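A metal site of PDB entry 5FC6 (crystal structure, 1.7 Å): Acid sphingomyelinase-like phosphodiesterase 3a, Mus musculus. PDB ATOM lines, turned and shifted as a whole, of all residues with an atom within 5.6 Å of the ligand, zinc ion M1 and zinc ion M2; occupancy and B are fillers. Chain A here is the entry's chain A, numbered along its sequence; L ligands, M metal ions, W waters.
NE2 of His 99 is in hydrogen-bond range of O1 of the ligand, 2.5 Å away.
An oxygen (O5) of the ligand lies within hydrogen-bond range of a ring nitrogen (NE2) of His 137 (3.1 Å).
The backbone NH (N) of His 278 lies within hydrogen-bond range of the side-chain carboxylate (OD1) of Asp 30.
O of Asp 30 sits at hydrogen-bond distance from N of Thr 305 (3.4 Å).
The side-chain carboxylate (OD1) of Asp 143 is in hydrogen-bond range of the side-chain amide nitrogen (ND2) of Asn 136 (2.8 Å).
The side-chain carboxylate of Asp 95 lies within hydrogen-bond range of the backbone NH of His 137, at 2.9 Å.
The backbone NH (N) of Arg 281 sits close to the side-chain hydroxyl (OG1) of Thr 279, at 3.2 Å.
Tyr 199 touches the ligand (OH to C2, 3.5 Å).
OH of Tyr 245 touches C8 of the ligand, 3.5 Å away.
Arg 281 touches the ligand.
Gln 312 touches the ligand.
13 residues have an atom within 4 Å of the ligand: Asp 30, His 32, Asp 95, His 99, Asn 136, His 137, Tyr 199, His 237, Tyr 245, His 278, His 280, Arg 281 and Gln 312.
Along chain A the residues within 4 Å of the ligand span positions 30 to 312.
Of the 20 residues printed, 4 come within 4 Å of zinc ion M1.
The side-chain carboxylate (OD2) of Asp 30 binds zinc ion M1.
O3 of the ligand binds zinc ion M1, 2.1 Å away.
Zinc ion M1 is bound by a ring nitrogen (NE2) of His 32 (2.1 Å).
Zinc ion M1 is bound by a ring nitrogen (NE2) of His 280, 2.2 Å away.
OD2 of Asp 95 binds zinc ion M1 (2.4 Å).
Zinc ion M1 has five donor atoms within binding distance.
Slightly farther from zinc ion M1 lies O1 of the ligand (2.6 Å).
Zinc ion M2 is bound by the side-chain amide oxygen (OD1) of Asn 136 (2.1 Å), a ring nitrogen (NE2) of His 237 (2.1 Å), an oxygen (O2) of the ligand (2.2 Å), a ring nitrogen (ND1) of His 278 (2.2 Å), an oxygen (O3) of the ligand (2.3 Å) and the side-chain carboxylate (OD2) of Asp 95 (2.4 Å).
Zinc ion M2 has six donor atoms within binding distance.
Water W2 lies within hydrogen-bond range of O5 of the ligand (2.8 Å), NE2 of Gln 142 (3.0 Å) and NE2 of His 137 (3.5 Å).
Water W4 lies within hydrogen-bond range of N3 of the ligand (2.8 Å), OH of Tyr 395 (2.9 Å) and NE of Arg 281 (3.0 Å).
Water W5 lies within hydrogen-bond range of O of Thr 279 (2.7 Å) and N3 of the ligand (2.9 Å).
Water W6 bridges OH of Tyr 245 and O7 of the ligand.
Water W3 lies within hydrogen-bond range of O of His 278 (2.7 Å) and N2 of the ligand (3.2 Å).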
ATOM      1  N   ASP A  30     -17.208 -26.904 -16.152  1.00  0.00           N
ATOM      2  CA  ASP A  30     -16.058 -26.519 -16.968  1.00  0.00           C
ATOM      3  C   ASP A  30     -15.579 -27.695 -17.817  1.00  0.00           C
ATOM      4  O   ASP A  30     -14.428 -28.126 -17.743  1.00  0.00           O
ATOM      5  CB  ASP A  30     -14.947 -25.949 -16.089  1.00  0.00           C
ATOM      6  CG  ASP A  30     -15.318 -24.567 -15.530  1.00  0.00           C
ATOM      7  OD1 ASP A  30     -15.856 -24.521 -14.395  1.00  0.00           O
ATOM      8  OD2 ASP A  30     -15.098 -23.553 -16.238  1.00  0.00           O
ATOM      9  N   HIS A  32     -15.424 -27.806 -21.202  1.00  0.00           N
ATOM     10  CA  HIS A  32     -14.564 -27.250 -22.262  1.00  0.00           C
ATOM     11  C   HIS A  32     -14.176 -28.314 -23.289  1.00  0.00           C
ATOM     12  O   HIS A  32     -13.017 -28.670 -23.450  1.00  0.00           O
ATOM     13  CB  HIS A  32     -13.295 -26.603 -21.683  1.00  0.00           C
ATOM     14  CG  HIS A  32     -13.557 -25.365 -20.890  1.00  0.00           C
ATOM     15  ND1 HIS A  32     -13.962 -24.172 -21.454  1.00  0.00           N
ATOM     16  CD2 HIS A  32     -13.434 -25.142 -19.560  1.00  0.00           C
ATOM     17  CE1 HIS A  32     -14.071 -23.253 -20.496  1.00  0.00           C
ATOM     18  NE2 HIS A  32     -13.757 -23.818 -19.347  1.00  0.00           N
ATOM     19  N   ASP A  95     -19.495 -23.452 -19.056  1.00  0.00           N
ATOM     20  CA  ASP A  95     -18.238 -23.363 -19.820  1.00  0.00           C
ATOM     21  C   ASP A  95     -17.959 -24.591 -20.680  1.00  0.00           C
ATOM     22  O   ASP A  95     -17.068 -25.401 -20.378  1.00  0.00           O
ATOM     23  CB  ASP A  95     -17.062 -23.097 -18.872  1.00  0.00           C
ATOM     24  CG  ASP A  95     -16.636 -21.643 -18.850  1.00  0.00           C
ATOM     25  OD1 ASP A  95     -17.346 -20.797 -19.425  1.00  0.00           O
ATOM     26  OD2 ASP A  95     -15.536 -21.382 -18.273  1.00  0.00           O
ATOM     27  N   HIS A  99     -11.074 -23.138 -25.219  1.00  0.00           N
ATOM     28  CA  HIS A  99     -10.305 -21.900 -25.157  1.00  0.00           C
ATOM     29  C   HIS A  99      -9.560 -21.714 -26.479  1.00  0.00           C
ATOM     30  O   HIS A  99      -8.417 -22.174 -26.645  1.00  0.00           O
ATOM     31  CB  HIS A  99      -9.310 -21.932 -24.011  1.00  0.00           C
ATOM     32  CG  HIS A  99      -9.946 -22.070 -22.654  1.00  0.00           C
ATOM     33  ND1 HIS A  99     -10.321 -23.301 -22.143  1.00  0.00           N
ATOM     34  CD2 HIS A  99     -10.253 -21.152 -21.709  1.00  0.00           C
ATOM     35  CE1 HIS A  99     -10.839 -23.122 -20.927  1.00  0.00           C
ATOM     36  NE2 HIS A  99     -10.814 -21.837 -20.642  1.00  0.00           N
ATOM     37  N   GLY A 135     -21.742 -20.368 -18.423  1.00  0.00           N
ATOM     38  CA  GLY A 135     -20.393 -19.858 -18.177  1.00  0.00           C
ATOM     39  C   GLY A 135     -20.038 -18.744 -19.155  1.00  0.00           C
ATOM     40  O   GLY A 135     -20.736 -18.457 -20.123  1.00  0.00           O
ATOM     41  N   ASN A 136     -18.885 -18.112 -18.898  1.00  0.00           N
ATOM     42  CA  ASN A 136     -18.480 -16.980 -19.722  1.00  0.00           C
ATOM     43  C   ASN A 136     -18.061 -17.408 -21.126  1.00  0.00           C
ATOM     44  O   ASN A 136     -18.116 -16.589 -22.050  1.00  0.00           O
ATOM     45  CB  ASN A 136     -17.352 -16.195 -19.019  1.00  0.00           C
ATOM     46  CG  ASN A 136     -16.162 -17.081 -18.629  1.00  0.00           C
ATOM     47  OD1 ASN A 136     -16.286 -17.994 -17.814  1.00  0.00           O
ATOM     48  ND2 ASN A 136     -15.028 -16.861 -19.280  1.00  0.00           N
ATOM     49  N   HIS A 137     -17.656 -18.659 -21.315  1.00  0.00           N
ATOM     50  CA  HIS A 137     -17.359 -19.146 -22.647  1.00  0.00           C
ATOM     51  C   HIS A 137     -18.609 -19.631 -23.358  1.00  0.00           C
ATOM     52  O   HIS A 137     -18.525 -19.990 -24.542  1.00  0.00           O
ATOM     53  CB  HIS A 137     -16.318 -20.265 -22.586  1.00  0.00           C
ATOM     54  CG  HIS A 137     -14.954 -19.780 -22.223  1.00  0.00           C
ATOM     55  ND1 HIS A 137     -14.037 -19.368 -23.176  1.00  0.00           N
ATOM     56  CD2 HIS A 137     -14.354 -19.591 -21.017  1.00  0.00           C
ATOM     57  CE1 HIS A 137     -12.921 -18.973 -22.559  1.00  0.00           C
ATOM     58  NE2 HIS A 137     -13.088 -19.115 -21.259  1.00  0.00           N
ATOM     59  N   GLN A 142     -16.762 -14.669 -26.465  1.00  0.00           N
ATOM     60  CA  GLN A 142     -16.703 -15.059 -25.069  1.00  0.00           C
ATOM     61  C   GLN A 142     -16.783 -13.836 -24.175  1.00  0.00           C
ATOM     62  O   GLN A 142     -16.334 -12.737 -24.521  1.00  0.00           O
ATOM     63  CB  GLN A 142     -15.414 -15.846 -24.779  1.00  0.00           C
ATOM     64  CG  GLN A 142     -14.126 -15.060 -24.825  1.00  0.00           C
ATOM     65  CD  GLN A 142     -12.954 -15.868 -24.274  1.00  0.00           C
ATOM     66  OE1 GLN A 142     -12.370 -16.727 -24.952  1.00  0.00           O
ATOM     67  NE2 GLN A 142     -12.623 -15.622 -23.001  1.00  0.00           N
ATOM     68  N   ASP A 143     -17.394 -14.051 -23.011  1.00  0.00           N
ATOM     69  CA  ASP A 143     -17.501 -13.142 -21.886  1.00  0.00           C
ATOM     70  C   ASP A 143     -18.530 -12.032 -22.133  1.00  0.00           C
ATOM     71  O   ASP A 143     -18.846 -11.315 -21.193  1.00  0.00           O
ATOM     72  CB  ASP A 143     -16.165 -12.480 -21.518  1.00  0.00           C
ATOM     73  CG  ASP A 143     -15.029 -13.464 -21.346  1.00  0.00           C
ATOM     74  OD1 ASP A 143     -15.260 -14.624 -20.925  1.00  0.00           O
ATOM     75  OD2 ASP A 143     -13.870 -13.069 -21.627  1.00  0.00           O
ATOM     76  N   TYR A 199     -18.748 -10.239 -14.573  1.00  0.00           N
ATOM     77  CA  TYR A 199     -17.346 -10.628 -14.814  1.00  0.00           C
ATOM     78  C   TYR A 199     -16.621  -9.520 -15.576  1.00  0.00           C
ATOM     79  O   TYR A 199     -17.139  -8.931 -16.525  1.00  0.00           O
ATOM     80  CB  TYR A 199     -17.353 -11.957 -15.579  1.00  0.00           C
ATOM     81  CG  TYR A 199     -16.034 -12.569 -15.892  1.00  0.00           C
ATOM     82  CD1 TYR A 199     -15.040 -12.710 -14.918  1.00  0.00           C
ATOM     83  CD2 TYR A 199     -15.793 -13.100 -17.153  1.00  0.00           C
ATOM     84  CE1 TYR A 199     -13.860 -13.307 -15.214  1.00  0.00           C
ATOM     85  CE2 TYR A 199     -14.593 -13.695 -17.463  1.00  0.00           C
ATOM     86  CZ  TYR A 199     -13.632 -13.797 -16.493  1.00  0.00           C
ATOM     87  OH  TYR A 199     -12.444 -14.399 -16.800  1.00  0.00           O
ATOM     88  N   HIS A 237     -21.573 -19.771 -12.441  1.00  0.00           N
ATOM     89  CA  HIS A 237     -20.253 -20.044 -12.997  1.00  0.00           C
ATOM     90  C   HIS A 237     -19.142 -19.297 -12.252  1.00  0.00           C
ATOM     91  O   HIS A 237     -18.324 -19.917 -11.567  1.00  0.00           O
ATOM     92  CB  HIS A 237     -20.230 -19.707 -14.485  1.00  0.00           C
ATOM     93  CG  HIS A 237     -18.930 -20.071 -15.121  1.00  0.00           C
ATOM     94  ND1 HIS A 237     -18.500 -21.385 -15.207  1.00  0.00           N
ATOM     95  CD2 HIS A 237     -17.937 -19.313 -15.615  1.00  0.00           C
ATOM     96  CE1 HIS A 237     -17.303 -21.401 -15.772  1.00  0.00           C
ATOM     97  NE2 HIS A 237     -16.947 -20.166 -16.043  1.00  0.00           N
ATOM     98  N   VAL A 238     -19.075 -17.978 -12.406  1.00  0.00           N
ATOM     99  CA  VAL A 238     -18.016 -17.201 -11.753  1.00  0.00           C
ATOM    100  C   VAL A 238     -18.362 -17.045 -10.277  1.00  0.00           C
ATOM    101  O   VAL A 238     -19.508 -16.694  -9.961  1.00  0.00           O
ATOM    102  CB  VAL A 238     -17.827 -15.836 -12.401  1.00  0.00           C
ATOM    103  CG1 VAL A 238     -16.616 -15.102 -11.782  1.00  0.00           C
ATOM    104  CG2 VAL A 238     -17.655 -15.978 -13.896  1.00  0.00           C
ATOM    105  N   TYR A 245      -5.179 -17.082  -5.766  1.00  0.00           N
ATOM    106  CA  TYR A 245      -3.807 -17.116  -6.291  1.00  0.00           C
ATOM    107  C   TYR A 245      -3.269 -15.742  -6.640  1.00  0.00           C
ATOM    108  O   TYR A 245      -2.150 -15.637  -7.139  1.00  0.00           O
ATOM    109  CB  TYR A 245      -3.738 -18.006  -7.539  1.00  0.00           C
ATOM    110  CG  TYR A 245      -4.663 -17.539  -8.659  1.00  0.00           C
ATOM    111  CD1 TYR A 245      -5.951 -18.059  -8.767  1.00  0.00           C
ATOM    112  CD2 TYR A 245      -4.274 -16.562  -9.570  1.00  0.00           C
ATOM    113  CE1 TYR A 245      -6.806 -17.653  -9.739  1.00  0.00           C
ATOM    114  CE2 TYR A 245      -5.147 -16.130 -10.576  1.00  0.00           C
ATOM    115  CZ  TYR A 245      -6.419 -16.686 -10.647  1.00  0.00           C
ATOM    116  OH  TYR A 245      -7.313 -16.313 -11.616  1.00  0.00           O
ATOM    117  N   HIS A 278     -15.644 -22.082 -12.805  1.00  0.00           N
ATOM    118  CA  HIS A 278     -14.775 -21.074 -13.420  1.00  0.00           C
ATOM    119  C   HIS A 278     -13.297 -21.095 -13.031  1.00  0.00           C
ATOM    120  O   HIS A 278     -12.432 -20.766 -13.864  1.00  0.00           O
ATOM    121  CB  HIS A 278     -15.331 -19.674 -13.118  1.00  0.00           C
ATOM    122  CG  HIS A 278     -14.554 -18.568 -13.762  1.00  0.00           C
ATOM    123  ND1 HIS A 278     -14.539 -18.346 -15.130  1.00  0.00           N
ATOM    124  CD2 HIS A 278     -13.804 -17.580 -13.216  1.00  0.00           C
ATOM    125  CE1 HIS A 278     -13.783 -17.293 -15.387  1.00  0.00           C
ATOM    126  NE2 HIS A 278     -13.313 -16.817 -14.248  1.00  0.00           N
ATOM    127  N   THR A 279     -12.960 -21.395 -11.779  1.00  0.00           N
ATOM    128  CA  THR A 279     -11.559 -21.307 -11.403  1.00  0.00           C
ATOM    129  C   THR A 279     -10.779 -22.565 -11.781  1.00  0.00           C
ATOM    130  O   THR A 279      -9.545 -22.544 -11.811  1.00  0.00           O
ATOM    131  CB  THR A 279     -11.421 -21.092  -9.888  1.00  0.00           C
ATOM    132  OG1 THR A 279     -11.737 -22.302  -9.245  1.00  0.00           O
ATOM    133  CG2 THR A 279     -12.321 -19.986  -9.385  1.00  0.00           C
ATOM    134  N   HIS A 280     -11.478 -23.652 -12.053  1.00  0.00           N
ATOM    135  CA  HIS A 280     -10.865 -24.941 -12.368  1.00  0.00           C
ATOM    136  C   HIS A 280     -10.073 -25.497 -11.219  1.00  0.00           C
ATOM    137  O   HIS A 280      -9.181 -26.337 -11.397  1.00  0.00           O
ATOM    138  CB  HIS A 280      -9.975 -24.858 -13.636  1.00  0.00           C
ATOM    139  CG  HIS A 280     -10.701 -24.493 -14.897  1.00  0.00           C
ATOM    140  ND1 HIS A 280     -10.191 -24.776 -16.151  1.00  0.00           N
ATOM    141  CD2 HIS A 280     -11.878 -23.869 -15.105  1.00  0.00           C
ATOM    142  CE1 HIS A 280     -11.016 -24.310 -17.068  1.00  0.00           C
ATOM    143  NE2 HIS A 280     -12.059 -23.770 -16.468  1.00  0.00           N
ATOM    144  N   ARG A 281     -10.385 -25.069 -10.006  1.00  0.00           N
ATOM    145  CA  ARG A 281      -9.663 -25.506  -8.822  1.00  0.00           C
ATOM    146  C   ARG A 281     -10.675 -25.921  -7.761  1.00  0.00           C
ATOM    147  O   ARG A 281     -11.835 -25.536  -7.813  1.00  0.00           O
ATOM    148  CB  ARG A 281      -8.766 -24.389  -8.264  1.00  0.00           C
ATOM    149  CG  ARG A 281      -7.707 -23.905  -9.223  1.00  0.00           C
ATOM    150  CD  ARG A 281      -6.576 -24.911  -9.388  1.00  0.00           C
ATOM    151  NE  ARG A 281      -5.564 -24.418 -10.311  1.00  0.00           N
ATOM    152  CZ  ARG A 281      -5.551 -24.644 -11.619  1.00  0.00           C
ATOM    153  NH1 ARG A 281      -6.490 -25.378 -12.205  1.00  0.00           N
ATOM    154  NH2 ARG A 281      -4.597 -24.120 -12.354  1.00  0.00           N
ATOM    155  N   THR A 305     -11.921 -30.366 -17.715  1.00  0.00           N
ATOM    156  CA  THR A 305     -10.737 -30.052 -18.529  1.00  0.00           C
ATOM    157  C   THR A 305      -9.501 -29.898 -17.637  1.00  0.00           C
ATOM    158  O   THR A 305      -9.581 -29.335 -16.520  1.00  0.00           O
ATOM    159  CB  THR A 305     -10.934 -28.792 -19.387  1.00  0.00           C
ATOM    160  OG1 THR A 305      -9.797 -28.614 -20.236  1.00  0.00           O
ATOM    161  CG2 THR A 305     -11.086 -27.508 -18.528  1.00  0.00           C
ATOM    162  N   GLN A 312       1.868 -21.293 -16.977  1.00  0.00           N
ATOM    163  CA  GLN A 312       1.469 -21.785 -15.678  1.00  0.00           C
ATOM    164  C   GLN A 312       2.257 -23.025 -15.326  1.00  0.00           C
ATOM    165  O   GLN A 312       2.448 -23.908 -16.158  1.00  0.00           O
ATOM    166  CB  GLN A 312      -0.031 -22.127 -15.650  1.00  0.00           C
ATOM    167  CG  GLN A 312      -0.955 -20.951 -15.834  1.00  0.00           C
ATOM    168  CD  GLN A 312      -2.416 -21.408 -15.972  1.00  0.00           C
ATOM    169  OE1 GLN A 312      -2.961 -21.455 -17.073  1.00  0.00           O
ATOM    170  NE2 GLN A 312      -3.019 -21.785 -14.855  1.00  0.00           N
ATOM    171  N   TYR A 395      -6.276 -28.612  -3.961  1.00  0.00           N
ATOM    172  CA  TYR A 395      -6.624 -27.440  -4.756  1.00  0.00           C
ATOM    173  C   TYR A 395      -6.377 -27.693  -6.248  1.00  0.00           C
ATOM    174  O   TYR A 395      -7.202 -27.337  -7.098  1.00  0.00           O
ATOM    175  CB  TYR A 395      -5.824 -26.252  -4.211  1.00  0.00           C
ATOM    176  CG  TYR A 395      -5.846 -24.973  -5.006  1.00  0.00           C
ATOM    177  CD1 TYR A 395      -6.967 -24.152  -5.018  1.00  0.00           C
ATOM    178  CD2 TYR A 395      -4.715 -24.542  -5.704  1.00  0.00           C
ATOM    179  CE1 TYR A 395      -6.981 -22.952  -5.744  1.00  0.00           C
ATOM    180  CE2 TYR A 395      -4.731 -23.345  -6.440  1.00  0.00           C
ATOM    181  CZ  TYR A 395      -5.849 -22.554  -6.446  1.00  0.00           C
ATOM    182  OH  TYR A 395      -5.850 -21.388  -7.166  1.00  0.00           O
HETATM  183  P1  LIG L   1     -12.626 -20.081 -17.699  1.00  0.00           P
HETATM  184  O1  LIG L   1     -12.235 -21.078 -18.753  1.00  0.00           O
HETATM  185  O2  LIG L   1     -13.492 -18.953 -18.140  1.00  0.00           O
HETATM  186  O3  LIG L   1     -13.417 -20.909 -16.608  1.00  0.00           O
HETATM  187  C1  LIG L   1     -11.185 -19.398 -16.791  1.00  0.00           C
HETATM  188  P2  LIG L   1     -10.012 -18.793 -18.084  1.00  0.00           P
HETATM  189  O4  LIG L   1      -9.091 -19.944 -18.455  1.00  0.00           O
HETATM  190  O5  LIG L   1     -10.898 -18.398 -19.246  1.00  0.00           O
HETATM  191  O6  LIG L   1      -9.059 -17.605 -17.448  1.00  0.00           O
HETATM  192  C2  LIG L   1      -9.484 -16.338 -17.052  1.00  0.00           C
HETATM  193  C3  LIG L   1      -8.261 -15.467 -16.911  1.00  0.00           C
HETATM  194  O7  LIG L   1      -7.698 -15.577 -15.746  1.00  0.00           O
HETATM  195  C4  LIG L   1      -7.089 -15.926 -18.024  1.00  0.00           C
HETATM  196  O8  LIG L   1      -6.360 -14.748 -18.471  1.00  0.00           O
HETATM  197  C5  LIG L   1      -6.298 -16.743 -17.426  1.00  0.00           C
HETATM  198  O9  LIG L   1      -4.908 -16.616 -17.969  1.00  0.00           O
HETATM  199  C6  LIG L   1      -6.328 -16.331 -15.910  1.00  0.00           C
HETATM  200  N1  LIG L   1      -6.273 -17.335 -15.048  1.00  0.00           N
HETATM  201  C7  LIG L   1      -7.304 -18.122 -14.780  1.00  0.00           C
HETATM  202  N2  LIG L   1      -6.977 -19.014 -13.859  1.00  0.00           N
HETATM  203  C8  LIG L   1      -5.708 -18.825 -13.497  1.00  0.00           C
HETATM  204  C9  LIG L   1      -4.841 -19.457 -12.569  1.00  0.00           C
HETATM  205  N3  LIG L   1      -5.348 -20.574 -11.775  1.00  0.00           N
HETATM  206  N4  LIG L   1      -3.588 -19.005 -12.430  1.00  0.00           N
HETATM  207  C10 LIG L   1      -3.170 -17.971 -13.172  1.00  0.00           C
HETATM  208  N5  LIG L   1      -3.976 -17.362 -14.052  1.00  0.00           N
HETATM  209  C11 LIG L   1      -5.251 -17.758 -14.241  1.00  0.00           C
HETATM  210 ZN    ZN M   1     -13.730 -22.802 -17.490  1.00  0.00          ZN
HETATM  211 ZN    ZN M   2     -15.208 -19.480 -16.898  1.00  0.00          ZN
HETATM  212  O   HOH W   1      -1.268 -18.781 -10.366  1.00  0.00           O
HETATM  213  O   HOH W   2     -10.385 -16.960 -21.564  1.00  0.00           O
HETATM  214  O   HOH W   3     -10.160 -19.277 -13.892  1.00  0.00           O
HETATM  215  O   HOH W   4      -4.248 -21.862  -9.551  1.00  0.00           O
HETATM  216  O   HOH W   5      -8.099 -20.463 -10.807  1.00  0.00           O
HETATM  217  O   HOH W   6      -6.725 -14.272 -13.139  1.00  0.00           O
